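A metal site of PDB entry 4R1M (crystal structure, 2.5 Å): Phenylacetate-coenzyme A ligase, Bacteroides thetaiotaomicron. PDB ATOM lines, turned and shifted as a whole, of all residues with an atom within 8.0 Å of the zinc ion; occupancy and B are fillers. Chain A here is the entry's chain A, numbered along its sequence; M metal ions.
The side-chain hydroxyl (OG1) of Thr 4 lies close to the backbone carbonyl oxygen (O) of Cys 316 (3.5 Å). The backbone carbonyl oxygen (O) of Cys 316 is in hydrogen-bond range of the side-chain hydroxyl (OH) of Tyr 6, 2.8 Å away. The guanidinium group (NH1) of Arg 318 sits close to the side-chain sulfur (SG) of Cys 316 (3.2 Å). N of His 259 sits at hydrogen-bond distance from O of Phe 250 (2.9 Å). The side-chain sulfur (SG) of Cys 252 sits close to the backbone NH (N) of Glu 254 (3.5 Å). ND1 of His 259 lies within hydrogen-bond range of O of His 320 (2.8 Å).
The nearest printed residue that does not touch the zinc ion is Arg 322 (4.6 Å).
The zinc ion is bound by a ring nitrogen (NE2) of His 259 (2.1 Å), the side-chain sulfur (SG) of Cys 316 (2.2 Å), the side-chain sulfur (SG) of Cys 252 (2.3 Å) and the side-chain sulfur (SG) of Cys 314 (2.3 Å). The zinc ion has four donor atoms within binding distance.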
ATOM      1  N   THR A   4       0.536 -35.028   3.998  1.00  0.00           N
ATOM      2  CA  THR A   4       1.986 -34.768   4.160  1.00  0.00           C
ATOM      3  C   THR A   4       2.521 -35.322   5.503  1.00  0.00           C
ATOM      4  O   THR A   4       1.878 -35.167   6.551  1.00  0.00           O
ATOM      5  CB  THR A   4       2.298 -33.239   4.057  1.00  0.00           C
ATOM      6  OG1 THR A   4       1.671 -32.708   2.890  1.00  0.00           O
ATOM      7  CG2 THR A   4       3.790 -32.951   3.957  1.00  0.00           C
ATOM      8  N   TYR A   6       6.023 -35.466   8.057  1.00  0.00           N
ATOM      9  CA  TYR A   6       7.208 -34.726   8.452  1.00  0.00           C
ATOM     10  C   TYR A   6       8.111 -35.519   9.357  1.00  0.00           C
ATOM     11  O   TYR A   6       7.628 -36.304  10.173  1.00  0.00           O
ATOM     12  CB  TYR A   6       6.798 -33.433   9.177  1.00  0.00           C
ATOM     13  CG  TYR A   6       5.687 -32.665   8.491  1.00  0.00           C
ATOM     14  CD1 TYR A   6       5.958 -31.772   7.460  1.00  0.00           C
ATOM     15  CD2 TYR A   6       4.348 -32.849   8.853  1.00  0.00           C
ATOM     16  CE1 TYR A   6       4.938 -31.076   6.815  1.00  0.00           C
ATOM     17  CE2 TYR A   6       3.326 -32.162   8.219  1.00  0.00           C
ATOM     18  CZ  TYR A   6       3.618 -31.277   7.193  1.00  0.00           C
ATOM     19  OH  TYR A   6       2.609 -30.602   6.570  1.00  0.00           O
ATOM     20  N   MET A 124      11.254 -35.999   3.677  1.00  0.00           N
ATOM     21  CA  MET A 124      10.331 -35.051   3.011  1.00  0.00           C
ATOM     22  C   MET A 124       9.970 -35.500   1.596  1.00  0.00           C
ATOM     23  O   MET A 124       8.826 -35.312   1.165  1.00  0.00           O
ATOM     24  CB  MET A 124      10.991 -33.659   2.971  1.00  0.00           C
ATOM     25  CG  MET A 124      10.220 -32.608   2.177  1.00  0.00           C
ATOM     26  SD  MET A 124      10.945 -30.798   2.455  1.00  0.00           S
ATOM     27  CE  MET A 124      12.702 -31.027   1.769  1.00  0.00           C
ATOM     28  N   PHE A 250      16.273 -28.149   0.047  1.00  0.00           N
ATOM     29  CA  PHE A 250      15.827 -29.304  -0.699  1.00  0.00           C
ATOM     30  C   PHE A 250      14.389 -29.140  -1.106  1.00  0.00           C
ATOM     31  O   PHE A 250      13.602 -28.586  -0.331  1.00  0.00           O
ATOM     32  CB  PHE A 250      15.985 -30.498   0.276  1.00  0.00           C
ATOM     33  CG  PHE A 250      16.360 -31.859  -0.217  1.00  0.00           C
ATOM     34  CD1 PHE A 250      15.383 -32.771  -0.626  1.00  0.00           C
ATOM     35  CD2 PHE A 250      17.684 -32.289  -0.193  1.00  0.00           C
ATOM     36  CE1 PHE A 250      15.728 -34.064  -1.032  1.00  0.00           C
ATOM     37  CE2 PHE A 250      18.025 -33.605  -0.562  1.00  0.00           C
ATOM     38  CZ  PHE A 250      17.046 -34.474  -0.999  1.00  0.00           C
ATOM     39  N   GLU A 251      14.032 -29.609  -2.306  1.00  0.00           N
ATOM     40  CA  GLU A 251      12.649 -29.564  -2.807  1.00  0.00           C
ATOM     41  C   GLU A 251      11.746 -30.448  -1.991  1.00  0.00           C
ATOM     42  O   GLU A 251      12.197 -31.475  -1.485  1.00  0.00           O
ATOM     43  CB  GLU A 251      12.541 -29.990  -4.274  1.00  0.00           C
ATOM     44  CG  GLU A 251      12.943 -28.968  -5.305  1.00  0.00           C
ATOM     45  CD  GLU A 251      12.739 -29.429  -6.751  1.00  0.00           C
ATOM     46  OE1 GLU A 251      12.983 -30.623  -7.029  1.00  0.00           O
ATOM     47  OE2 GLU A 251      12.405 -28.574  -7.592  1.00  0.00           O
ATOM     48  N   CYS A 252      10.479 -30.079  -1.886  1.00  0.00           N
ATOM     49  CA  CYS A 252       9.484 -30.943  -1.256  1.00  0.00           C
ATOM     50  C   CYS A 252       8.821 -31.738  -2.378  1.00  0.00           C
ATOM     51  O   CYS A 252       9.264 -31.622  -3.522  1.00  0.00           O
ATOM     52  CB  CYS A 252       8.482 -30.156  -0.415  1.00  0.00           C
ATOM     53  SG  CYS A 252       7.461 -28.992  -1.374  1.00  0.00           S
ATOM     54  N   GLN A 253       7.760 -32.494  -2.117  1.00  0.00           N
ATOM     55  CA  GLN A 253       7.111 -33.295  -3.150  1.00  0.00           C
ATOM     56  C   GLN A 253       6.351 -32.414  -4.169  1.00  0.00           C
ATOM     57  O   GLN A 253       5.965 -32.945  -5.212  1.00  0.00           O
ATOM     58  CB  GLN A 253       6.189 -34.350  -2.544  1.00  0.00           C
ATOM     59  CG  GLN A 253       7.028 -35.377  -1.788  1.00  0.00           C
ATOM     60  CD  GLN A 253       6.263 -36.584  -1.356  1.00  0.00           C
ATOM     61  OE1 GLN A 253       5.401 -37.090  -2.075  1.00  0.00           O
ATOM     62  NE2 GLN A 253       6.620 -37.129  -0.203  1.00  0.00           N
ATOM     63  N   GLU A 254       6.254 -31.099  -3.938  1.00  0.00           N
ATOM     64  CA  GLU A 254       5.651 -30.119  -4.872  1.00  0.00           C
ATOM     65  C   GLU A 254       6.609 -29.765  -6.024  1.00  0.00           C
ATOM     66  O   GLU A 254       6.163 -29.230  -7.028  1.00  0.00           O
ATOM     67  CB  GLU A 254       5.236 -28.816  -4.170  1.00  0.00           C
ATOM     68  CG  GLU A 254       4.071 -28.976  -3.206  1.00  0.00           C
ATOM     69  CD  GLU A 254       2.752 -29.346  -3.861  1.00  0.00           C
ATOM     70  OE1 GLU A 254       2.372 -28.699  -4.862  1.00  0.00           O
ATOM     71  OE2 GLU A 254       2.094 -30.279  -3.346  1.00  0.00           O
ATOM     72  N   GLN A 255       7.934 -30.042  -5.842  1.00  0.00           N
ATOM     73  CA  GLN A 255       9.003 -29.760  -6.827  1.00  0.00           C
ATOM     74  C   GLN A 255       8.894 -28.315  -7.321  1.00  0.00           C
ATOM     75  O   GLN A 255       8.975 -28.053  -8.521  1.00  0.00           O
ATOM     76  CB  GLN A 255       8.956 -30.740  -8.008  1.00  0.00           C
ATOM     77  CG  GLN A 255       9.242 -32.179  -7.604  1.00  0.00           C
ATOM     78  CD  GLN A 255       9.125 -33.108  -8.764  1.00  0.00           C
ATOM     79  OE1 GLN A 255       8.098 -33.148  -9.475  1.00  0.00           O
ATOM     80  NE2 GLN A 255      10.132 -33.960  -8.915  1.00  0.00           N
ATOM     81  N   ASN A 256       8.707 -27.378  -6.391  1.00  0.00           N
ATOM     82  CA  ASN A 256       8.577 -25.954  -6.697  1.00  0.00           C
ATOM     83  C   ASN A 256       9.274 -25.134  -5.627  1.00  0.00           C
ATOM     84  O   ASN A 256       8.637 -24.676  -4.664  1.00  0.00           O
ATOM     85  CB  ASN A 256       7.094 -25.571  -6.843  1.00  0.00           C
ATOM     86  CG  ASN A 256       6.835 -24.116  -7.207  1.00  0.00           C
ATOM     87  OD1 ASN A 256       5.832 -23.533  -6.781  1.00  0.00           O
ATOM     88  ND2 ASN A 256       7.771 -23.495  -7.963  1.00  0.00           N
ATOM     89  N   GLY A 257      10.580 -24.951  -5.821  1.00  0.00           N
ATOM     90  CA  GLY A 257      11.423 -24.213  -4.896  1.00  0.00           C
ATOM     91  C   GLY A 257      12.015 -25.127  -3.844  1.00  0.00           C
ATOM     92  O   GLY A 257      11.434 -26.168  -3.531  1.00  0.00           O
ATOM     93  N   MET A 258      13.179 -24.766  -3.333  1.00  0.00           N
ATOM     94  CA  MET A 258      13.867 -25.585  -2.333  1.00  0.00           C
ATOM     95  C   MET A 258      13.689 -24.979  -0.957  1.00  0.00           C
ATOM     96  O   MET A 258      14.071 -23.822  -0.728  1.00  0.00           O
ATOM     97  CB  MET A 258      15.352 -25.721  -2.677  1.00  0.00           C
ATOM     98  CG  MET A 258      15.592 -26.530  -3.927  1.00  0.00           C
ATOM     99  SD  MET A 258      17.449 -26.652  -4.397  1.00  0.00           S
ATOM    100  CE  MET A 258      17.852 -24.891  -4.962  1.00  0.00           C
ATOM    101  N   HIS A 259      13.058 -25.748  -0.044  1.00  0.00           N
ATOM    102  CA  HIS A 259      12.879 -25.328   1.345  1.00  0.00           C
ATOM    103  C   HIS A 259      14.212 -25.211   2.037  1.00  0.00           C
ATOM    104  O   HIS A 259      14.996 -26.163   2.025  1.00  0.00           O
ATOM    105  CB  HIS A 259      11.988 -26.295   2.117  1.00  0.00           C
ATOM    106  CG  HIS A 259      10.549 -26.194   1.758  1.00  0.00           C
ATOM    107  ND1 HIS A 259       9.735 -25.218   2.331  1.00  0.00           N
ATOM    108  CD2 HIS A 259       9.803 -26.955   0.936  1.00  0.00           C
ATOM    109  CE1 HIS A 259       8.534 -25.406   1.820  1.00  0.00           C
ATOM    110  NE2 HIS A 259       8.509 -26.440   0.984  1.00  0.00           N
ATOM    111  N   TRP A 261      16.217 -24.837   5.512  1.00  0.00           N
ATOM    112  CA  TRP A 261      15.921 -25.118   6.926  1.00  0.00           C
ATOM    113  C   TRP A 261      16.389 -23.936   7.785  1.00  0.00           C
ATOM    114  O   TRP A 261      17.563 -23.801   8.125  1.00  0.00           O
ATOM    115  CB  TRP A 261      16.553 -26.444   7.374  1.00  0.00           C
ATOM    116  CG  TRP A 261      16.026 -27.608   6.566  1.00  0.00           C
ATOM    117  CD1 TRP A 261      16.743 -28.404   5.735  1.00  0.00           C
ATOM    118  CD2 TRP A 261      14.643 -27.956   6.364  1.00  0.00           C
ATOM    119  NE1 TRP A 261      15.916 -29.314   5.115  1.00  0.00           N
ATOM    120  CE2 TRP A 261      14.611 -29.047   5.458  1.00  0.00           C
ATOM    121  CE3 TRP A 261      13.416 -27.456   6.856  1.00  0.00           C
ATOM    122  CZ2 TRP A 261      13.424 -29.689   5.093  1.00  0.00           C
ATOM    123  CZ3 TRP A 261      12.233 -28.074   6.455  1.00  0.00           C
ATOM    124  CH2 TRP A 261      12.246 -29.183   5.608  1.00  0.00           C
ATOM    125  N   LYS A 313       2.831 -19.238   0.397  1.00  0.00           N
ATOM    126  CA  LYS A 313       2.842 -20.437   1.224  1.00  0.00           C
ATOM    127  C   LYS A 313       2.978 -21.652   0.326  1.00  0.00           C
ATOM    128  O   LYS A 313       2.506 -21.606  -0.818  1.00  0.00           O
ATOM    129  CB  LYS A 313       1.569 -20.509   2.090  1.00  0.00           C
ATOM    130  CG  LYS A 313       1.445 -19.393   3.111  1.00  0.00           C
ATOM    131  CD  LYS A 313       0.228 -19.553   4.006  1.00  0.00           C
ATOM    132  CE  LYS A 313       0.144 -18.460   5.050  1.00  0.00           C
ATOM    133  NZ  LYS A 313      -0.970 -18.696   6.005  1.00  0.00           N
ATOM    134  N   CYS A 314       3.626 -22.729   0.810  1.00  0.00           N
ATOM    135  CA  CYS A 314       3.764 -23.934   0.015  1.00  0.00           C
ATOM    136  C   CYS A 314       2.626 -24.890   0.344  1.00  0.00           C
ATOM    137  O   CYS A 314       2.353 -25.072   1.537  1.00  0.00           O
ATOM    138  CB  CYS A 314       5.130 -24.613   0.196  1.00  0.00           C
ATOM    139  SG  CYS A 314       5.365 -26.076  -0.852  1.00  0.00           S
ATOM    140  N   PRO A 315       2.018 -25.588  -0.649  1.00  0.00           N
ATOM    141  CA  PRO A 315       0.957 -26.569  -0.324  1.00  0.00           C
ATOM    142  C   PRO A 315       1.436 -27.733   0.566  1.00  0.00           C
ATOM    143  O   PRO A 315       0.587 -28.423   1.110  1.00  0.00           O
ATOM    144  CB  PRO A 315       0.521 -27.104  -1.684  1.00  0.00           C
ATOM    145  CG  PRO A 315       0.975 -26.102  -2.669  1.00  0.00           C
ATOM    146  CD  PRO A 315       2.224 -25.506  -2.107  1.00  0.00           C
ATOM    147  N   CYS A 316       2.763 -27.976   0.743  1.00  0.00           N
ATOM    148  CA  CYS A 316       3.191 -29.103   1.582  1.00  0.00           C
ATOM    149  C   CYS A 316       2.943 -28.748   3.077  1.00  0.00           C
ATOM    150  O   CYS A 316       2.934 -29.633   3.919  1.00  0.00           O
ATOM    151  CB  CYS A 316       4.656 -29.510   1.333  1.00  0.00           C
ATOM    152  SG  CYS A 316       5.903 -28.403   2.054  1.00  0.00           S
ATOM    153  N   GLY A 317       2.698 -27.467   3.353  1.00  0.00           N
ATOM    154  CA  GLY A 317       2.422 -26.976   4.688  1.00  0.00           C
ATOM    155  C   GLY A 317       3.647 -26.510   5.459  1.00  0.00           C
ATOM    156  O   GLY A 317       3.500 -26.010   6.577  1.00  0.00           O
ATOM    157  N   ARG A 318       4.861 -26.656   4.902  1.00  0.00           N
ATOM    158  CA  ARG A 318       6.070 -26.208   5.580  1.00  0.00           C
ATOM    159  C   ARG A 318       6.189 -24.694   5.464  1.00  0.00           C
ATOM    160  O   ARG A 318       5.855 -24.101   4.445  1.00  0.00           O
ATOM    161  CB  ARG A 318       7.327 -26.918   5.039  1.00  0.00           C
ATOM    162  CG  ARG A 318       7.330 -28.402   5.377  1.00  0.00           C
ATOM    163  CD  ARG A 318       8.474 -29.127   4.712  1.00  0.00           C
ATOM    164  NE  ARG A 318       8.489 -30.548   5.044  1.00  0.00           N
ATOM    165  CZ  ARG A 318       7.813 -31.479   4.374  1.00  0.00           C
ATOM    166  NH1 ARG A 318       7.064 -31.147   3.331  1.00  0.00           N
ATOM    167  NH2 ARG A 318       7.894 -32.743   4.735  1.00  0.00           N
ATOM    168  N   THR A 319       6.613 -24.074   6.575  1.00  0.00           N
ATOM    169  CA  THR A 319       6.711 -22.633   6.780  1.00  0.00           C
ATOM    170  C   THR A 319       8.121 -22.090   6.502  1.00  0.00           C
ATOM    171  O   THR A 319       8.322 -20.874   6.521  1.00  0.00           O
ATOM    172  CB  THR A 319       6.307 -22.319   8.231  1.00  0.00           C
ATOM    173  OG1 THR A 319       7.048 -23.214   9.110  1.00  0.00           O
ATOM    174  CG2 THR A 319       4.792 -22.509   8.459  1.00  0.00           C
ATOM    175  N   HIS A 320       9.088 -22.981   6.263  1.00  0.00           N
ATOM    176  CA  HIS A 320      10.459 -22.619   5.937  1.00  0.00           C
ATOM    177  C   HIS A 320      10.495 -22.093   4.524  1.00  0.00           C
ATOM    178  O   HIS A 320       9.908 -22.715   3.623  1.00  0.00           O
ATOM    179  CB  HIS A 320      11.387 -23.832   6.136  1.00  0.00           C
ATOM    180  CG  HIS A 320      11.515 -24.236   7.556  1.00  0.00           C
ATOM    181  ND1 HIS A 320      12.689 -24.033   8.263  1.00  0.00           N
ATOM    182  CD2 HIS A 320      10.580 -24.770   8.382  1.00  0.00           C
ATOM    183  CE1 HIS A 320      12.451 -24.482   9.491  1.00  0.00           C
ATOM    184  NE2 HIS A 320      11.196 -24.916   9.607  1.00  0.00           N
ATOM    185  N   ARG A 322      11.351 -20.931   0.669  1.00  0.00           N
ATOM    186  CA  ARG A 322      11.809 -21.628  -0.537  1.00  0.00           C
ATOM    187  C   ARG A 322      12.667 -20.722  -1.387  1.00  0.00           C
ATOM    188  O   ARG A 322      12.331 -19.556  -1.570  1.00  0.00           O
ATOM    189  CB  ARG A 322      10.622 -22.151  -1.392  1.00  0.00           C
ATOM    190  CG  ARG A 322       9.813 -23.240  -0.712  1.00  0.00           C
ATOM    191  CD  ARG A 322       8.477 -23.495  -1.394  1.00  0.00           C
ATOM    192  NE  ARG A 322       7.635 -22.289  -1.405  1.00  0.00           N
ATOM    193  CZ  ARG A 322       7.334 -21.605  -2.498  1.00  0.00           C
ATOM    194  NH1 ARG A 322       7.741 -22.019  -3.685  1.00  0.00           N
ATOM    195  NH2 ARG A 322       6.591 -20.515  -2.411  1.00  0.00           N
HETATM  196 ZN    ZN M   1       6.868 -27.505   0.250  1.00  0.00          ZN
